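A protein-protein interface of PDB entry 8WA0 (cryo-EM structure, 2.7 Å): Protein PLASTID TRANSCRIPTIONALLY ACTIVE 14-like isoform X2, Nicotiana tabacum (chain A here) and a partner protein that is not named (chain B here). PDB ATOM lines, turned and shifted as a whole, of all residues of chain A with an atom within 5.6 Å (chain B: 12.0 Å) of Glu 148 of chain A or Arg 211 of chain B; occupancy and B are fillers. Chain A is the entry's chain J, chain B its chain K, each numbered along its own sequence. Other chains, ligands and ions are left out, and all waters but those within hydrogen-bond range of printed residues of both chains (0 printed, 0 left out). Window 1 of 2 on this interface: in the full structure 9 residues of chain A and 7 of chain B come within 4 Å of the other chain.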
ATOM      1  N   ARG A 109     -20.962  26.068 -33.770  1.00  0.00           N
ATOM      2  CA  ARG A 109     -19.900  25.279 -33.174  1.00  0.00           C
ATOM      3  C   ARG A 109     -19.736  24.260 -34.269  1.00  0.00           C
ATOM      4  O   ARG A 109     -20.469  24.262 -35.214  1.00  0.00           O
ATOM      5  CB  ARG A 109     -20.365  24.641 -31.900  1.00  0.00           C
ATOM      6  CG  ARG A 109     -20.258  25.525 -30.673  1.00  0.00           C
ATOM      7  CD  ARG A 109     -21.473  26.410 -30.510  1.00  0.00           C
ATOM      8  NE  ARG A 109     -21.512  27.017 -29.189  1.00  0.00           N
ATOM      9  CZ  ARG A 109     -22.442  27.877 -28.796  1.00  0.00           C
ATOM     10  NH1 ARG A 109     -23.406  28.235 -29.630  1.00  0.00           N
ATOM     11  NH2 ARG A 109     -22.401  28.382 -27.574  1.00  0.00           N
ATOM     12  N   SER A 110     -18.778  23.379 -34.224  1.00  0.00           N
ATOM     13  CA  SER A 110     -18.663  22.511 -35.387  1.00  0.00           C
ATOM     14  C   SER A 110     -19.519  21.250 -35.483  1.00  0.00           C
ATOM     15  O   SER A 110     -18.981  20.174 -35.633  1.00  0.00           O
ATOM     16  CB  SER A 110     -17.209  22.163 -35.619  1.00  0.00           C
ATOM     17  OG  SER A 110     -17.033  21.570 -36.887  1.00  0.00           O
ATOM     18  N   PRO A 146     -18.836  17.268 -32.020  1.00  0.00           N
ATOM     19  CA  PRO A 146     -17.538  17.398 -31.365  1.00  0.00           C
ATOM     20  C   PRO A 146     -17.534  17.144 -29.868  1.00  0.00           C
ATOM     21  O   PRO A 146     -18.582  17.178 -29.259  1.00  0.00           O
ATOM     22  CB  PRO A 146     -17.189  18.853 -31.606  1.00  0.00           C
ATOM     23  CG  PRO A 146     -18.070  19.325 -32.689  1.00  0.00           C
ATOM     24  CD  PRO A 146     -19.331  18.601 -32.419  1.00  0.00           C
ATOM     25  N   LEU A 147     -16.373  16.901 -29.279  1.00  0.00           N
ATOM     26  CA  LEU A 147     -16.269  16.609 -27.852  1.00  0.00           C
ATOM     27  C   LEU A 147     -16.680  17.738 -26.947  1.00  0.00           C
ATOM     28  O   LEU A 147     -17.291  17.513 -25.917  1.00  0.00           O
ATOM     29  CB  LEU A 147     -14.863  16.164 -27.490  1.00  0.00           C
ATOM     30  CG  LEU A 147     -14.514  15.797 -26.048  1.00  0.00           C
ATOM     31  CD1 LEU A 147     -15.334  14.615 -25.564  1.00  0.00           C
ATOM     32  CD2 LEU A 147     -13.033  15.494 -25.934  1.00  0.00           C
ATOM     33  N   GLU A 148     -16.361  18.961 -27.310  1.00  0.00           N
ATOM     34  CA  GLU A 148     -16.641  20.089 -26.443  1.00  0.00           C
ATOM     35  C   GLU A 148     -18.111  20.275 -26.149  1.00  0.00           C
ATOM     36  O   GLU A 148     -18.470  20.687 -25.059  1.00  0.00           O
ATOM     37  CB  GLU A 148     -16.026  21.359 -27.002  1.00  0.00           C
ATOM     38  CG  GLU A 148     -16.564  21.812 -28.342  1.00  0.00           C
ATOM     39  CD  GLU A 148     -15.600  21.553 -29.476  1.00  0.00           C
ATOM     40  OE1 GLU A 148     -14.635  20.787 -29.281  1.00  0.00           O
ATOM     41  OE2 GLU A 148     -15.817  22.118 -30.565  1.00  0.00           O
ATOM     42  N   LEU A 149     -18.970  20.000 -27.110  1.00  0.00           N
ATOM     43  CA  LEU A 149     -20.395  20.095 -26.889  1.00  0.00           C
ATOM     44  C   LEU A 149     -20.879  19.121 -25.817  1.00  0.00           C
ATOM     45  O   LEU A 149     -21.792  19.441 -25.083  1.00  0.00           O
ATOM     46  CB  LEU A 149     -21.132  19.883 -28.197  1.00  0.00           C
ATOM     47  CG  LEU A 149     -21.438  21.070 -29.108  1.00  0.00           C
ATOM     48  CD1 LEU A 149     -20.210  21.908 -29.388  1.00  0.00           C
ATOM     49  CD2 LEU A 149     -22.068  20.601 -30.406  1.00  0.00           C
ATOM     50  N   MET A 150     -20.234  17.977 -25.657  1.00  0.00           N
ATOM     51  CA  MET A 150     -20.696  16.949 -24.720  1.00  0.00           C
ATOM     52  C   MET A 150     -20.333  17.099 -23.260  1.00  0.00           C
ATOM     53  O   MET A 150     -19.558  17.970 -22.926  1.00  0.00           O
ATOM     54  CB  MET A 150     -20.165  15.611 -25.200  1.00  0.00           C
ATOM     55  CG  MET A 150     -20.486  15.297 -26.646  1.00  0.00           C
ATOM     56  SD  MET A 150     -19.320  14.131 -27.365  1.00  0.00           S
ATOM     57  CE  MET A 150     -19.018  13.066 -25.967  1.00  0.00           C
ATOM     58  N   PRO A 163     -14.594  17.053 -21.038  1.00  0.00           N
ATOM     59  CA  PRO A 163     -14.768  18.427 -21.512  1.00  0.00           C
ATOM     60  C   PRO A 163     -14.192  19.334 -20.422  1.00  0.00           C
ATOM     61  O   PRO A 163     -13.846  20.452 -20.754  1.00  0.00           O
ATOM     62  CB  PRO A 163     -16.258  18.549 -21.675  1.00  0.00           C
ATOM     63  CG  PRO A 163     -16.681  17.161 -22.014  1.00  0.00           C
ATOM     64  CD  PRO A 163     -15.835  16.277 -21.155  1.00  0.00           C
ATOM     65  N   ASP A 324      -9.960  13.733 -34.552  1.00  0.00           N
ATOM     66  CA  ASP A 324     -10.593  14.999 -34.556  1.00  0.00           C
ATOM     67  C   ASP A 324     -11.439  15.102 -33.336  1.00  0.00           C
ATOM     68  O   ASP A 324     -12.231  16.013 -33.231  1.00  0.00           O
ATOM     69  CB  ASP A 324     -11.477  15.020 -35.757  1.00  0.00           C
ATOM     70  CG  ASP A 324     -10.702  14.996 -37.054  1.00  0.00           C
ATOM     71  OD1 ASP A 324      -9.478  15.242 -37.027  1.00  0.00           O
ATOM     72  OD2 ASP A 324     -11.319  14.740 -38.110  1.00  0.00           O
ATOM     73  N   ARG A 325     -11.337  14.174 -32.427  1.00  0.00           N
ATOM     74  CA  ARG A 325     -12.108  14.150 -31.206  1.00  0.00           C
ATOM     75  C   ARG A 325     -13.594  14.235 -31.324  1.00  0.00           C
ATOM     76  O   ARG A 325     -14.207  14.976 -30.601  1.00  0.00           O
ATOM     77  CB  ARG A 325     -11.445  14.981 -30.142  1.00  0.00           C
ATOM     78  CG  ARG A 325      -9.940  14.848 -30.174  1.00  0.00           C
ATOM     79  CD  ARG A 325      -9.364  14.534 -28.820  1.00  0.00           C
ATOM     80  NE  ARG A 325      -9.254  15.722 -28.002  1.00  0.00           N
ATOM     81  CZ  ARG A 325      -8.148  16.090 -27.378  1.00  0.00           C
ATOM     82  NH1 ARG A 325      -7.056  15.363 -27.479  1.00  0.00           N
ATOM     83  NH2 ARG A 325      -8.139  17.186 -26.643  1.00  0.00           N
ATOM     84  N   MET A 326     -14.193  13.450 -32.197  1.00  0.00           N
ATOM     85  CA  MET A 326     -15.614  13.485 -32.476  1.00  0.00           C
ATOM     86  C   MET A 326     -16.419  12.215 -32.438  1.00  0.00           C
ATOM     87  O   MET A 326     -15.866  11.166 -32.656  1.00  0.00           O
ATOM     88  CB  MET A 326     -15.816  14.084 -33.867  1.00  0.00           C
ATOM     89  CG  MET A 326     -15.516  15.565 -33.952  1.00  0.00           C
ATOM     90  SD  MET A 326     -16.120  16.417 -35.414  1.00  0.00           S
ATOM     91  CE  MET A 326     -15.149  15.620 -36.683  1.00  0.00           C
ATOM     92  N   PRO B 205      -4.227  31.973 -26.296  1.00  0.00           N
ATOM     93  CA  PRO B 205      -4.081  30.885 -25.372  1.00  0.00           C
ATOM     94  C   PRO B 205      -3.492  29.664 -25.985  1.00  0.00           C
ATOM     95  O   PRO B 205      -3.609  29.483 -27.188  1.00  0.00           O
ATOM     96  CB  PRO B 205      -5.508  30.600 -25.010  1.00  0.00           C
ATOM     97  CG  PRO B 205      -6.329  30.989 -26.165  1.00  0.00           C
ATOM     98  CD  PRO B 205      -5.552  32.005 -26.931  1.00  0.00           C
ATOM     99  N   PRO B 206      -2.854  28.804 -25.207  1.00  0.00           N
ATOM    100  CA  PRO B 206      -2.198  27.648 -25.803  1.00  0.00           C
ATOM    101  C   PRO B 206      -3.154  26.658 -26.513  1.00  0.00           C
ATOM    102  O   PRO B 206      -4.191  26.385 -25.949  1.00  0.00           O
ATOM    103  CB  PRO B 206      -1.506  27.050 -24.612  1.00  0.00           C
ATOM    104  CG  PRO B 206      -1.204  28.189 -23.726  1.00  0.00           C
ATOM    105  CD  PRO B 206      -2.449  29.003 -23.809  1.00  0.00           C
ATOM    106  N   ILE B 207      -2.830  26.130 -27.701  1.00  0.00           N
ATOM    107  CA  ILE B 207      -3.719  25.234 -28.475  1.00  0.00           C
ATOM    108  C   ILE B 207      -3.389  23.757 -28.340  1.00  0.00           C
ATOM    109  O   ILE B 207      -2.356  23.311 -28.798  1.00  0.00           O
ATOM    110  CB  ILE B 207      -3.736  25.590 -29.966  1.00  0.00           C
ATOM    111  CG1 ILE B 207      -4.044  27.063 -30.164  1.00  0.00           C
ATOM    112  CG2 ILE B 207      -4.753  24.757 -30.718  1.00  0.00           C
ATOM    113  CD1 ILE B 207      -4.220  27.444 -31.612  1.00  0.00           C
ATOM    114  N   ASP B 208      -4.267  22.986 -27.710  1.00  0.00           N
ATOM    115  CA  ASP B 208      -4.013  21.569 -27.451  1.00  0.00           C
ATOM    116  C   ASP B 208      -4.901  20.533 -28.074  1.00  0.00           C
ATOM    117  O   ASP B 208      -4.738  19.359 -27.795  1.00  0.00           O
ATOM    118  CB  ASP B 208      -4.053  21.327 -25.957  1.00  0.00           C
ATOM    119  CG  ASP B 208      -2.721  21.587 -25.287  1.00  0.00           C
ATOM    120  OD1 ASP B 208      -1.803  22.104 -25.954  1.00  0.00           O
ATOM    121  OD2 ASP B 208      -2.590  21.267 -24.087  1.00  0.00           O
ATOM    122  N   ALA B 209      -5.818  20.915 -28.912  1.00  0.00           N
ATOM    123  CA  ALA B 209      -6.741  19.997 -29.455  1.00  0.00           C
ATOM    124  C   ALA B 209      -7.050  20.511 -30.780  1.00  0.00           C
ATOM    125  O   ALA B 209      -6.719  21.631 -31.099  1.00  0.00           O
ATOM    126  CB  ALA B 209      -7.983  20.000 -28.611  1.00  0.00           C
ATOM    127  N   PRO B 210      -7.716  19.682 -31.632  1.00  0.00           N
ATOM    128  CA  PRO B 210      -7.912  20.223 -32.972  1.00  0.00           C
ATOM    129  C   PRO B 210      -8.659  21.532 -33.103  1.00  0.00           C
ATOM    130  O   PRO B 210      -8.163  22.354 -33.814  1.00  0.00           O
ATOM    131  CB  PRO B 210      -8.652  19.113 -33.699  1.00  0.00           C
ATOM    132  CG  PRO B 210      -9.255  18.277 -32.638  1.00  0.00           C
ATOM    133  CD  PRO B 210      -8.198  18.280 -31.592  1.00  0.00           C
ATOM    134  N   ARG B 211      -9.790  21.764 -32.475  1.00  0.00           N
ATOM    135  CA  ARG B 211     -10.476  23.034 -32.720  1.00  0.00           C
ATOM    136  C   ARG B 211     -10.368  24.054 -31.608  1.00  0.00           C
ATOM    137  O   ARG B 211     -11.168  24.970 -31.536  1.00  0.00           O
ATOM    138  CB  ARG B 211     -11.906  22.818 -33.185  1.00  0.00           C
ATOM    139  CG  ARG B 211     -12.749  21.942 -32.291  1.00  0.00           C
ATOM    140  CD  ARG B 211     -13.914  21.369 -33.073  1.00  0.00           C
ATOM    141  NE  ARG B 211     -13.466  20.401 -34.062  1.00  0.00           N
ATOM    142  CZ  ARG B 211     -13.313  19.106 -33.815  1.00  0.00           C
ATOM    143  NH1 ARG B 211     -13.570  18.618 -32.611  1.00  0.00           N
ATOM    144  NH2 ARG B 211     -12.901  18.301 -34.777  1.00  0.00           N
ATOM    145  N   ASP B 212      -9.395  23.892 -30.730  1.00  0.00           N
ATOM    146  CA  ASP B 212      -9.204  24.794 -29.601  1.00  0.00           C
ATOM    147  C   ASP B 212      -9.233  26.314 -29.893  1.00  0.00           C
ATOM    148  O   ASP B 212      -8.723  26.726 -30.921  1.00  0.00           O
ATOM    149  CB  ASP B 212      -7.904  24.430 -28.911  1.00  0.00           C
ATOM    150  CG  ASP B 212      -7.753  25.079 -27.556  1.00  0.00           C
ATOM    151  OD1 ASP B 212      -8.352  24.570 -26.588  1.00  0.00           O
ATOM    152  OD2 ASP B 212      -7.031  26.094 -27.453  1.00  0.00           O
ATOM    153  N   PRO B 213      -9.813  27.160 -28.990  1.00  0.00           N
ATOM    154  CA  PRO B 213      -9.870  28.572 -29.328  1.00  0.00           C
ATOM    155  C   PRO B 213      -8.586  29.342 -29.593  1.00  0.00           C
ATOM    156  O   PRO B 213      -7.673  29.259 -28.798  1.00  0.00           O
ATOM    157  CB  PRO B 213     -10.609  29.127 -28.178  1.00  0.00           C
ATOM    158  CG  PRO B 213     -11.558  28.071 -27.792  1.00  0.00           C
ATOM    159  CD  PRO B 213     -10.762  26.822 -27.924  1.00  0.00           C
ATOM    160  N   MET B 214      -8.505  30.070 -30.691  1.00  0.00           N
ATOM    161  CA  MET B 214      -7.351  30.879 -31.040  1.00  0.00           C
ATOM    162  C   MET B 214      -7.118  32.164 -30.285  1.00  0.00           C
ATOM    163  O   MET B 214      -6.008  32.641 -30.232  1.00  0.00           O
ATOM    164  CB  MET B 214      -7.277  31.119 -32.521  1.00  0.00           C
ATOM    165  CG  MET B 214      -6.765  29.905 -33.269  1.00  0.00           C
ATOM    166  SD  MET B 214      -6.072  30.176 -34.903  1.00  0.00           S
ATOM    167  CE  MET B 214      -4.505  30.922 -34.503  1.00  0.00           C
ATOM    168  N   TYR B 215      -8.165  32.743 -29.739  1.00  0.00           N
ATOM    169  CA  TYR B 215      -8.067  33.964 -29.019  1.00  0.00           C
ATOM    170  C   TYR B 215      -9.033  33.947 -27.869  1.00  0.00           C
ATOM    171  O   TYR B 215     -10.027  33.261 -27.944  1.00  0.00           O
ATOM    172  CB  TYR B 215      -8.366  35.096 -29.974  1.00  0.00           C
ATOM    173  CG  TYR B 215      -9.778  35.166 -30.487  1.00  0.00           C
ATOM    174  CD1 TYR B 215     -10.172  34.430 -31.590  1.00  0.00           C
ATOM    175  CD2 TYR B 215     -10.714  35.988 -29.885  1.00  0.00           C
ATOM    176  CE1 TYR B 215     -11.463  34.493 -32.061  1.00  0.00           C
ATOM    177  CE2 TYR B 215     -12.005  36.054 -30.347  1.00  0.00           C
ATOM    178  CZ  TYR B 215     -12.372  35.306 -31.436  1.00  0.00           C
ATOM    179  OH  TYR B 215     -13.660  35.372 -31.906  1.00  0.00           O
ATOM    180  N   LYS B 216      -8.784  34.729 -26.830  1.00  0.00           N
ATOM    181  CA  LYS B 216      -9.707  34.834 -25.719  1.00  0.00           C
ATOM    182  C   LYS B 216      -9.833  36.292 -25.357  1.00  0.00           C
ATOM    183  O   LYS B 216      -8.830  36.960 -25.199  1.00  0.00           O
ATOM    184  CB  LYS B 216      -9.159  34.075 -24.537  1.00  0.00           C
ATOM    185  CG  LYS B 216     -10.035  34.125 -23.304  1.00  0.00           C
ATOM    186  CD  LYS B 216      -9.356  33.437 -22.136  1.00  0.00           C
ATOM    187  CE  LYS B 216     -10.232  33.465 -20.896  1.00  0.00           C
ATOM    188  NZ  LYS B 216      -9.570  32.807 -19.737  1.00  0.00           N
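The backbone carbonyl oxygen of Asp 324 of chain A sits at hydrogen-bond distance from the guanidinium group of Arg 211 of chain B, at 2.8 Å. The guanidinium group of Arg 211 of chain B is in hydrogen-bond range of the side-chain sulfur of Met 326 of chain A (3.8 Å).
The backbone NH (N) of Leu 147 of chain A is in hydrogen-bond range of the backbone carbonyl oxygen (O) of Arg 325 of chain A.
Of the 11 printed residues of chain A, 5 touch a printed residue of chain B. Hydrophobic or aromatic side chains of chain A within 4 Å of the printed part of chain B: Pro 146 and Met 326. Hydrophobic or aromatic side chains of chain B within 4 Å of the printed part of chain A: Ala 209 and Pro 210.
NH1 of Arg 211 of chain B touches CB of Pro 146 of chain A (3.8 Å). CD of Arg 211 of chain B touches OE2 of Glu 148 of chain A (3.2 Å). Asp 324 of chain A touches Pro 210 of chain B. Arg 325 of chain A touches Ala 209 of chain B (NH2 to CB, 3.4 Å).
Glu 148 of chain A touches just one residue of chain B: Arg 211 (3.2 Å). Of chain A, only Pro 146, Glu 148, Asp 324 and Met 326 come within 4 Å of Arg 211 of chain B. No residue of chain B comes within 4 Å of Ser 110 of chain A. Met 150 of chain A touches none of the printed residues of chain B. No residue of chain B comes within 4 Å of Pro 163 of chain A. Met 326 of chain A touches one residue of chain B. Printed residues of chain A within 4 Å of Ala 209 of chain B: Arg 325. Of the printed residues of chain A, Pro 210 of chain B touches Asp 324 (3.8 Å). Pro 205 of chain B touches none of the printed residues of chain A. Pro 213 of chain B touches none of the printed residues of chain A. The nearest residue of chain B that does not touch Glu 148 of chain A is Asp 212 of chain B (6.3 Å). The nearest printed residue of chain B that does not touch Arg 325 of chain A is Pro 210 of chain B (4.1 Å).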
